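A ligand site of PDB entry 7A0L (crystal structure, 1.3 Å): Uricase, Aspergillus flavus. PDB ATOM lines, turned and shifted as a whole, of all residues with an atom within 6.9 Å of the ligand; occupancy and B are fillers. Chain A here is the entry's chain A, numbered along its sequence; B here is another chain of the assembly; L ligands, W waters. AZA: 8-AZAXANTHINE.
O2 of the ligand lies within hydrogen-bond range of N of Val 228 (2.9 Å). The side-chain amide nitrogen of Gln 229 is in hydrogen-bond range of an oxygen (O6) of the ligand (2.9 Å). ND2 of Asn 255 lies close to N3 of the ligand (3.3 Å). The side-chain hydroxyl (OG1) of Thr 58 of chain B sits at hydrogen-bond distance from a nitrogen (N7) of the ligand, at 3.3 Å. The backbone NH (N) of Thr 58 of chain B lies within hydrogen-bond range of a nitrogen (N7) of the ligand, 2.8 Å away. O2 of the ligand is in hydrogen-bond range of NH2 of Arg 177 (2.8 Å).
The backbone NH (N) of Arg 177 sits at hydrogen-bond distance from the backbone carbonyl oxygen (O) of Ser 158. The backbone NH (N) of Gln 229 lies close to the side-chain hydroxyl (OG) of Ser 227 (3.4 Å). The backbone carbonyl oxygen (O) of Val 56 of chain B sits at hydrogen-bond distance from the side-chain hydroxyl (OH) of Tyr 9 of chain B, 2.7 Å away. OG1 of Thr 58 of chain B lies within hydrogen-bond range of NZ of Lys 11 of chain B (2.9 Å). The backbone carbonyl oxygen (O) of Asn 255 is in hydrogen-bond range of a ring nitrogen (NE2) of His 257 (3.4 Å). The side-chain hydroxyl (OG) of Ser 225 is in hydrogen-bond range of the backbone carbonyl oxygen (O) of Ser 227 (3.0 Å). OG of Ser 227 lies within hydrogen-bond range of N of Ala 230 (2.9 Å). The backbone NH (N) of Asn 255 sits at hydrogen-bond distance from the backbone carbonyl oxygen (O) of Gly 287 (2.8 Å).
Residues that only touch the ligand: Phe 160, Leu 171, Ser 227, Tyr 9 of chain B, Ile 55 of chain B, Ala 57 of chain B and Asp 59 of chain B. Of the 27 residues printed, 12 come within 4 Å of the ligand.
Water W1 lies within hydrogen-bond range of a nitrogen (N9) of the ligand (2.8 Å) and the guanidinium group of Arg 177 (3.5 Å). Water W2 lies within hydrogen-bond range of OG1 of Thr 58 of chain B and ND2 of Asn 255.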
ATOM      1  N   SER A 158      15.258  -9.317  -5.670  1.00  0.00           N
ATOM      2  CA  SER A 158      15.694  -9.702  -6.995  1.00  0.00           C
ATOM      3  C   SER A 158      16.672 -10.849  -6.824  1.00  0.00           C
ATOM      4  O   SER A 158      17.557 -10.800  -5.949  1.00  0.00           O
ATOM      5  CB  SER A 158      16.364  -8.527  -7.689  1.00  0.00           C
ATOM      6  OG  SER A 158      16.952  -8.905  -8.926  1.00  0.00           O
ATOM      7  N   GLN A 159      16.487 -11.887  -7.639  1.00  0.00           N
ATOM      8  CA  GLN A 159      17.311 -13.087  -7.604  1.00  0.00           C
ATOM      9  C   GLN A 159      17.827 -13.371  -9.020  1.00  0.00           C
ATOM     10  O   GLN A 159      17.239 -12.942 -10.016  1.00  0.00           O
ATOM     11  CB  GLN A 159      16.477 -14.268  -7.107  1.00  0.00           C
ATOM     12  CG  GLN A 159      15.783 -14.003  -5.812  1.00  0.00           C
ATOM     13  CD  GLN A 159      15.108 -15.221  -5.203  1.00  0.00           C
ATOM     14  OE1 GLN A 159      15.239 -16.336  -5.671  1.00  0.00           O
ATOM     15  NE2 GLN A 159      14.394 -14.995  -4.136  1.00  0.00           N
ATOM     16  N   PHE A 160      18.888 -14.176  -9.102  1.00  0.00           N
ATOM     17  CA  PHE A 160      19.297 -14.690 -10.400  1.00  0.00           C
ATOM     18  C   PHE A 160      20.138 -15.939 -10.191  1.00  0.00           C
ATOM     19  O   PHE A 160      21.335 -15.872  -9.879  1.00  0.00           O
ATOM     20  CB  PHE A 160      19.999 -13.652 -11.275  1.00  0.00           C
ATOM     21  CG  PHE A 160      20.188 -14.119 -12.679  1.00  0.00           C
ATOM     22  CD1 PHE A 160      19.091 -14.384 -13.467  1.00  0.00           C
ATOM     23  CD2 PHE A 160      21.461 -14.291 -13.217  1.00  0.00           C
ATOM     24  CE1 PHE A 160      19.245 -14.807 -14.773  1.00  0.00           C
ATOM     25  CE2 PHE A 160      21.633 -14.735 -14.531  1.00  0.00           C
ATOM     26  CZ  PHE A 160      20.516 -15.007 -15.312  1.00  0.00           C
ATOM     27  N   PHE A 163      20.992 -20.398 -14.041  1.00  0.00           N
ATOM     28  CA  PHE A 163      21.377 -20.152 -15.417  1.00  0.00           C
ATOM     29  C   PHE A 163      22.434 -21.159 -15.851  1.00  0.00           C
ATOM     30  O   PHE A 163      23.023 -21.878 -15.047  1.00  0.00           O
ATOM     31  CB  PHE A 163      21.871 -18.708 -15.600  1.00  0.00           C
ATOM     32  CG  PHE A 163      22.900 -18.279 -14.579  1.00  0.00           C
ATOM     33  CD1 PHE A 163      22.522 -17.680 -13.399  1.00  0.00           C
ATOM     34  CD2 PHE A 163      24.238 -18.491 -14.805  1.00  0.00           C
ATOM     35  CE1 PHE A 163      23.462 -17.300 -12.439  1.00  0.00           C
ATOM     36  CE2 PHE A 163      25.183 -18.094 -13.885  1.00  0.00           C
ATOM     37  CZ  PHE A 163      24.797 -17.509 -12.700  1.00  0.00           C
ATOM     38  N   LEU A 171      30.027 -16.011 -13.199  1.00  0.00           N
ATOM     39  CA  LEU A 171      29.020 -15.377 -12.368  1.00  0.00           C
ATOM     40  C   LEU A 171      28.508 -16.338 -11.310  1.00  0.00           C
ATOM     41  O   LEU A 171      28.098 -17.460 -11.614  1.00  0.00           O
ATOM     42  CB  LEU A 171      27.875 -14.928 -13.265  1.00  0.00           C
ATOM     43  CG  LEU A 171      26.718 -14.185 -12.565  1.00  0.00           C
ATOM     44  CD1 LEU A 171      27.185 -12.853 -12.063  1.00  0.00           C
ATOM     45  CD2 LEU A 171      25.563 -13.984 -13.556  1.00  0.00           C
ATOM     46  N   ARG A 177      19.944  -9.539  -4.802  1.00  0.00           N
ATOM     47  CA  ARG A 177      20.779  -8.557  -5.489  1.00  0.00           C
ATOM     48  C   ARG A 177      19.981  -7.268  -5.692  1.00  0.00           C
ATOM     49  O   ARG A 177      18.754  -7.227  -5.523  1.00  0.00           O
ATOM     50  CB  ARG A 177      21.265  -9.085  -6.834  1.00  0.00           C
ATOM     51  CG  ARG A 177      20.148  -9.283  -7.847  1.00  0.00           C
ATOM     52  CD  ARG A 177      20.634  -9.763  -9.177  1.00  0.00           C
ATOM     53  NE  ARG A 177      19.489  -9.838 -10.098  1.00  0.00           N
ATOM     54  CZ  ARG A 177      19.593 -10.088 -11.398  1.00  0.00           C
ATOM     55  NH1 ARG A 177      20.763 -10.369 -11.935  1.00  0.00           N
ATOM     56  NH2 ARG A 177      18.511 -10.043 -12.163  1.00  0.00           N
ATOM     57  N   LEU A 179      18.507  -4.578  -8.278  1.00  0.00           N
ATOM     58  CA  LEU A 179      18.028  -4.525  -9.648  1.00  0.00           C
ATOM     59  C   LEU A 179      17.724  -3.078 -10.006  1.00  0.00           C
ATOM     60  O   LEU A 179      16.899  -2.439  -9.363  1.00  0.00           O
ATOM     61  CB  LEU A 179      16.786  -5.402  -9.839  1.00  0.00           C
ATOM     62  CG  LEU A 179      16.217  -5.470 -11.240  1.00  0.00           C
ATOM     63  CD1 LEU A 179      17.235  -5.937 -12.227  1.00  0.00           C
ATOM     64  CD2 LEU A 179      14.994  -6.372 -11.283  1.00  0.00           C
ATOM     65  N   SER A 225      11.692 -10.940  -8.158  1.00  0.00           N
ATOM     66  CA  SER A 225      12.094 -11.157  -9.537  1.00  0.00           C
ATOM     67  C   SER A 225      13.059 -12.320  -9.708  1.00  0.00           C
ATOM     68  O   SER A 225      14.102 -12.375  -9.069  1.00  0.00           O
ATOM     69  CB  SER A 225      12.749  -9.875 -10.029  1.00  0.00           C
ATOM     70  OG  SER A 225      13.303 -10.056 -11.318  1.00  0.00           O
ATOM     71  N   ALA A 226      12.709 -13.230 -10.611  1.00  0.00           N
ATOM     72  CA  ALA A 226      13.568 -14.356 -10.940  1.00  0.00           C
ATOM     73  C   ALA A 226      14.615 -14.025 -11.990  1.00  0.00           C
ATOM     74  O   ALA A 226      15.607 -14.760 -12.107  1.00  0.00           O
ATOM     75  CB  ALA A 226      12.694 -15.518 -11.443  1.00  0.00           C
ATOM     76  N   SER A 227      14.429 -12.920 -12.697  1.00  0.00           N
ATOM     77  CA  SER A 227      15.282 -12.415 -13.759  1.00  0.00           C
ATOM     78  C   SER A 227      14.592 -11.177 -14.318  1.00  0.00           C
ATOM     79  O   SER A 227      13.382 -10.982 -14.126  1.00  0.00           O
ATOM     80  CB  SER A 227      15.457 -13.420 -14.890  1.00  0.00           C
ATOM     81  OG  SER A 227      14.221 -13.638 -15.547  1.00  0.00           O
ATOM     82  N   VAL A 228      15.354 -10.379 -15.048  1.00  0.00           N
ATOM     83  CA  VAL A 228      14.747  -9.267 -15.774  1.00  0.00           C
ATOM     84  C   VAL A 228      13.702  -9.798 -16.738  1.00  0.00           C
ATOM     85  O   VAL A 228      12.612  -9.245 -16.882  1.00  0.00           O
ATOM     86  CB  VAL A 228      15.828  -8.438 -16.480  1.00  0.00           C
ATOM     87  CG1 VAL A 228      15.187  -7.362 -17.357  1.00  0.00           C
ATOM     88  CG2 VAL A 228      16.728  -7.792 -15.438  1.00  0.00           C
ATOM     89  N   GLN A 229      14.053 -10.878 -17.441  1.00  0.00           N
ATOM     90  CA  GLN A 229      13.172 -11.509 -18.414  1.00  0.00           C
ATOM     91  C   GLN A 229      11.797 -11.812 -17.818  1.00  0.00           C
ATOM     92  O   GLN A 229      10.753 -11.519 -18.410  1.00  0.00           O
ATOM     93  CB  GLN A 229      13.809 -12.818 -18.902  1.00  0.00           C
ATOM     94  CG  GLN A 229      15.022 -12.688 -19.835  1.00  0.00           C
ATOM     95  CD  GLN A 229      16.368 -12.527 -19.156  1.00  0.00           C
ATOM     96  OE1 GLN A 229      16.501 -12.070 -18.022  1.00  0.00           O
ATOM     97  NE2 GLN A 229      17.411 -12.886 -19.893  1.00  0.00           N
ATOM     98  N   ALA A 230      11.786 -12.472 -16.654  1.00  0.00           N
ATOM     99  CA  ALA A 230      10.527 -12.921 -16.078  1.00  0.00           C
ATOM    100  C   ALA A 230       9.681 -11.750 -15.608  1.00  0.00           C
ATOM    101  O   ALA A 230       8.467 -11.743 -15.767  1.00  0.00           O
ATOM    102  CB  ALA A 230      10.789 -13.877 -14.936  1.00  0.00           C
ATOM    103  N   ASN A 255      20.225  -3.875 -17.746  1.00  0.00           N
ATOM    104  CA  ASN A 255      20.490  -4.330 -16.373  1.00  0.00           C
ATOM    105  C   ASN A 255      21.718  -3.528 -15.920  1.00  0.00           C
ATOM    106  O   ASN A 255      22.822  -3.769 -16.379  1.00  0.00           O
ATOM    107  CB  ASN A 255      20.689  -5.845 -16.360  1.00  0.00           C
ATOM    108  CG  ASN A 255      20.694  -6.429 -14.989  1.00  0.00           C
ATOM    109  OD1 ASN A 255      20.519  -5.712 -14.002  1.00  0.00           O
ATOM    110  ND2 ASN A 255      20.841  -7.734 -14.909  1.00  0.00           N
ATOM    111  N   HIS A 257      24.355  -2.715 -13.480  1.00  0.00           N
ATOM    112  CA  HIS A 257      24.948  -3.532 -12.422  1.00  0.00           C
ATOM    113  C   HIS A 257      25.524  -2.699 -11.282  1.00  0.00           C
ATOM    114  O   HIS A 257      26.177  -1.686 -11.499  1.00  0.00           O
ATOM    115  CB  HIS A 257      26.052  -4.409 -13.000  1.00  0.00           C
ATOM    116  CG  HIS A 257      25.601  -5.253 -14.163  1.00  0.00           C
ATOM    117  ND1 HIS A 257      24.667  -6.253 -14.033  1.00  0.00           N
ATOM    118  CD2 HIS A 257      25.942  -5.223 -15.471  1.00  0.00           C
ATOM    119  CE1 HIS A 257      24.447  -6.808 -15.226  1.00  0.00           C
ATOM    120  NE2 HIS A 257      25.207  -6.205 -16.116  1.00  0.00           N
ATOM    121  N   GLY A 287      23.855  -5.326 -19.067  1.00  0.00           N
ATOM    122  CA  GLY A 287      22.962  -6.234 -19.729  1.00  0.00           C
ATOM    123  C   GLY A 287      21.903  -5.465 -20.504  1.00  0.00           C
ATOM    124  O   GLY A 287      21.575  -4.336 -20.194  1.00  0.00           O
ATOM    125  N   ILE A 289      18.097  -6.494 -22.224  1.00  0.00           N
ATOM    126  CA  ILE A 289      17.094  -7.547 -22.302  1.00  0.00           C
ATOM    127  C   ILE A 289      15.883  -6.973 -23.028  1.00  0.00           C
ATOM    128  O   ILE A 289      15.373  -5.933 -22.640  1.00  0.00           O
ATOM    129  CB  ILE A 289      16.676  -8.019 -20.906  1.00  0.00           C
ATOM    130  CG1 ILE A 289      17.863  -8.099 -19.937  1.00  0.00           C
ATOM    131  CG2 ILE A 289      15.995  -9.370 -21.009  1.00  0.00           C
ATOM    132  CD1 ILE A 289      18.907  -9.089 -20.293  1.00  0.00           C
ATOM    133  N   TYR B   9      18.528 -10.845 -26.097  1.00  0.00           N
ATOM    134  CA  TYR B   9      19.145 -10.363 -24.865  1.00  0.00           C
ATOM    135  C   TYR B   9      20.649 -10.534 -24.985  1.00  0.00           C
ATOM    136  O   TYR B   9      21.150 -11.369 -25.739  1.00  0.00           O
ATOM    137  CB  TYR B   9      18.603 -11.115 -23.637  1.00  0.00           C
ATOM    138  CG  TYR B   9      19.335 -12.401 -23.434  1.00  0.00           C
ATOM    139  CD1 TYR B   9      19.125 -13.485 -24.280  1.00  0.00           C
ATOM    140  CD2 TYR B   9      20.324 -12.513 -22.469  1.00  0.00           C
ATOM    141  CE1 TYR B   9      19.853 -14.646 -24.142  1.00  0.00           C
ATOM    142  CE2 TYR B   9      21.052 -13.673 -22.332  1.00  0.00           C
ATOM    143  CZ  TYR B   9      20.810 -14.727 -23.184  1.00  0.00           C
ATOM    144  OH  TYR B   9      21.545 -15.872 -23.069  1.00  0.00           O
ATOM    145  N   GLY B  10      21.378  -9.776 -24.194  1.00  0.00           N
ATOM    146  CA  GLY B  10      22.831  -9.917 -24.203  1.00  0.00           C
ATOM    147  C   GLY B  10      23.511  -8.808 -23.433  1.00  0.00           C
ATOM    148  O   GLY B  10      22.982  -8.300 -22.452  1.00  0.00           O
ATOM    149  N   LYS B  11      24.720  -8.480 -23.869  1.00  0.00           N
ATOM    150  CA  LYS B  11      25.557  -7.508 -23.162  1.00  0.00           C
ATOM    151  C   LYS B  11      25.893  -6.368 -24.117  1.00  0.00           C
ATOM    152  O   LYS B  11      26.306  -6.618 -25.249  1.00  0.00           O
ATOM    153  CB  LYS B  11      26.842  -8.147 -22.662  1.00  0.00           C
ATOM    154  CG  LYS B  11      27.508  -7.352 -21.556  1.00  0.00           C
ATOM    155  CD  LYS B  11      26.707  -7.435 -20.285  1.00  0.00           C
ATOM    156  CE  LYS B  11      27.433  -7.884 -19.093  1.00  0.00           C
ATOM    157  NZ  LYS B  11      26.497  -8.181 -18.003  1.00  0.00           N
ATOM    158  N   ASN B  52      15.569 -20.251 -15.996  1.00  0.00           N
ATOM    159  CA  ASN B  52      16.870 -19.680 -16.333  1.00  0.00           C
ATOM    160  C   ASN B  52      17.845 -20.667 -16.974  1.00  0.00           C
ATOM    161  O   ASN B  52      18.924 -20.242 -17.392  1.00  0.00           O
ATOM    162  CB  ASN B  52      17.487 -18.997 -15.115  1.00  0.00           C
ATOM    163  CG  ASN B  52      16.727 -17.767 -14.728  1.00  0.00           C
ATOM    164  OD1 ASN B  52      16.104 -17.107 -15.574  1.00  0.00           O
ATOM    165  ND2 ASN B  52      16.790 -17.410 -13.445  1.00  0.00           N
ATOM    166  N   ILE B  55      19.357 -19.629 -20.236  1.00  0.00           N
ATOM    167  CA  ILE B  55      20.054 -18.338 -20.302  1.00  0.00           C
ATOM    168  C   ILE B  55      21.560 -18.574 -20.218  1.00  0.00           C
ATOM    169  O   ILE B  55      22.068 -19.030 -19.178  1.00  0.00           O
ATOM    170  CB  ILE B  55      19.599 -17.396 -19.194  1.00  0.00           C
ATOM    171  CG1 ILE B  55      18.114 -17.061 -19.284  1.00  0.00           C
ATOM    172  CG2 ILE B  55      20.441 -16.091 -19.258  1.00  0.00           C
ATOM    173  CD1 ILE B  55      17.637 -16.105 -18.156  1.00  0.00           C
ATOM    174  N   VAL B  56      22.255 -18.210 -21.284  1.00  0.00           N
ATOM    175  CA  VAL B  56      23.695 -17.956 -21.256  1.00  0.00           C
ATOM    176  C   VAL B  56      23.823 -16.575 -20.613  1.00  0.00           C
ATOM    177  O   VAL B  56      23.350 -15.583 -21.150  1.00  0.00           O
ATOM    178  CB  VAL B  56      24.267 -17.965 -22.678  1.00  0.00           C
ATOM    179  CG1 VAL B  56      25.723 -17.634 -22.645  1.00  0.00           C
ATOM    180  CG2 VAL B  56      24.084 -19.364 -23.323  1.00  0.00           C
ATOM    181  N   ALA B  57      24.392 -16.507 -19.415  1.00  0.00           N
ATOM    182  CA  ALA B  57      24.330 -15.245 -18.674  1.00  0.00           C
ATOM    183  C   ALA B  57      25.012 -14.128 -19.449  1.00  0.00           C
ATOM    184  O   ALA B  57      26.011 -14.353 -20.143  1.00  0.00           O
ATOM    185  CB  ALA B  57      25.008 -15.420 -17.318  1.00  0.00           C
ATOM    186  N   THR B  58      24.489 -12.913 -19.308  1.00  0.00           N
ATOM    187  CA  THR B  58      25.104 -11.785 -20.007  1.00  0.00           C
ATOM    188  C   THR B  58      26.552 -11.591 -19.548  1.00  0.00           C
ATOM    189  O   THR B  58      27.413 -11.220 -20.337  1.00  0.00           O
ATOM    190  CB  THR B  58      24.279 -10.511 -19.884  1.00  0.00           C
ATOM    191  OG1 THR B  58      24.359  -9.986 -18.578  1.00  0.00           O
ATOM    192  CG2 THR B  58      22.817 -10.736 -20.298  1.00  0.00           C
ATOM    193  N   ASP B  59      26.819 -11.889 -18.280  1.00  0.00           N
ATOM    194  CA  ASP B  59      28.187 -11.829 -17.779  1.00  0.00           C
ATOM    195  C   ASP B  59      29.098 -12.807 -18.512  1.00  0.00           C
ATOM    196  O   ASP B  59      30.274 -12.497 -18.784  1.00  0.00           O
ATOM    197  CB  ASP B  59      28.178 -12.131 -16.279  1.00  0.00           C
ATOM    198  CG  ASP B  59      29.528 -11.903 -15.642  1.00  0.00           C
ATOM    199  OD1 ASP B  59      29.855 -10.718 -15.373  1.00  0.00           O
ATOM    200  OD2 ASP B  59      30.275 -12.879 -15.416  1.00  0.00           O
ATOM    201  N   SER B  60      28.588 -13.985 -18.859  1.00  0.00           N
ATOM    202  CA  SER B  60      29.336 -14.958 -19.632  1.00  0.00           C
ATOM    203  C   SER B  60      29.570 -14.503 -21.062  1.00  0.00           C
ATOM    204  O   SER B  60      30.604 -14.801 -21.654  1.00  0.00           O
ATOM    205  CB  SER B  60      28.623 -16.302 -19.616  1.00  0.00           C
ATOM    206  OG  SER B  60      28.404 -16.716 -18.278  1.00  0.00           O
HETATM  207  N1  AZA L   1      19.135 -11.734 -16.716  1.00  0.00           N
HETATM  208  C2  AZA L   1      19.240 -11.195 -15.428  1.00  0.00           C
HETATM  209  O2  AZA L   1      18.181 -10.821 -14.880  1.00  0.00           O
HETATM  210  N3  AZA L   1      20.476 -11.029 -14.833  1.00  0.00           N
HETATM  211  C4  AZA L   1      21.527 -11.520 -15.517  1.00  0.00           C
HETATM  212  C5  AZA L   1      21.463 -12.105 -16.789  1.00  0.00           C
HETATM  213  C6  AZA L   1      20.207 -12.208 -17.453  1.00  0.00           C
HETATM  214  O6  AZA L   1      20.010 -12.682 -18.601  1.00  0.00           O
HETATM  215  N7  AZA L   1      22.734 -12.475 -17.144  1.00  0.00           N
HETATM  216  N8  AZA L   1      23.596 -12.113 -16.167  1.00  0.00           N
HETATM  217  N9  AZA L   1      22.816 -11.556 -15.221  1.00  0.00           N
HETATM  218  O   HOH W   1      24.041 -10.284 -13.046  1.00  0.00           O
HETATM  219  O   HOH W   2      22.086  -8.751 -17.444  1.00  0.00           O
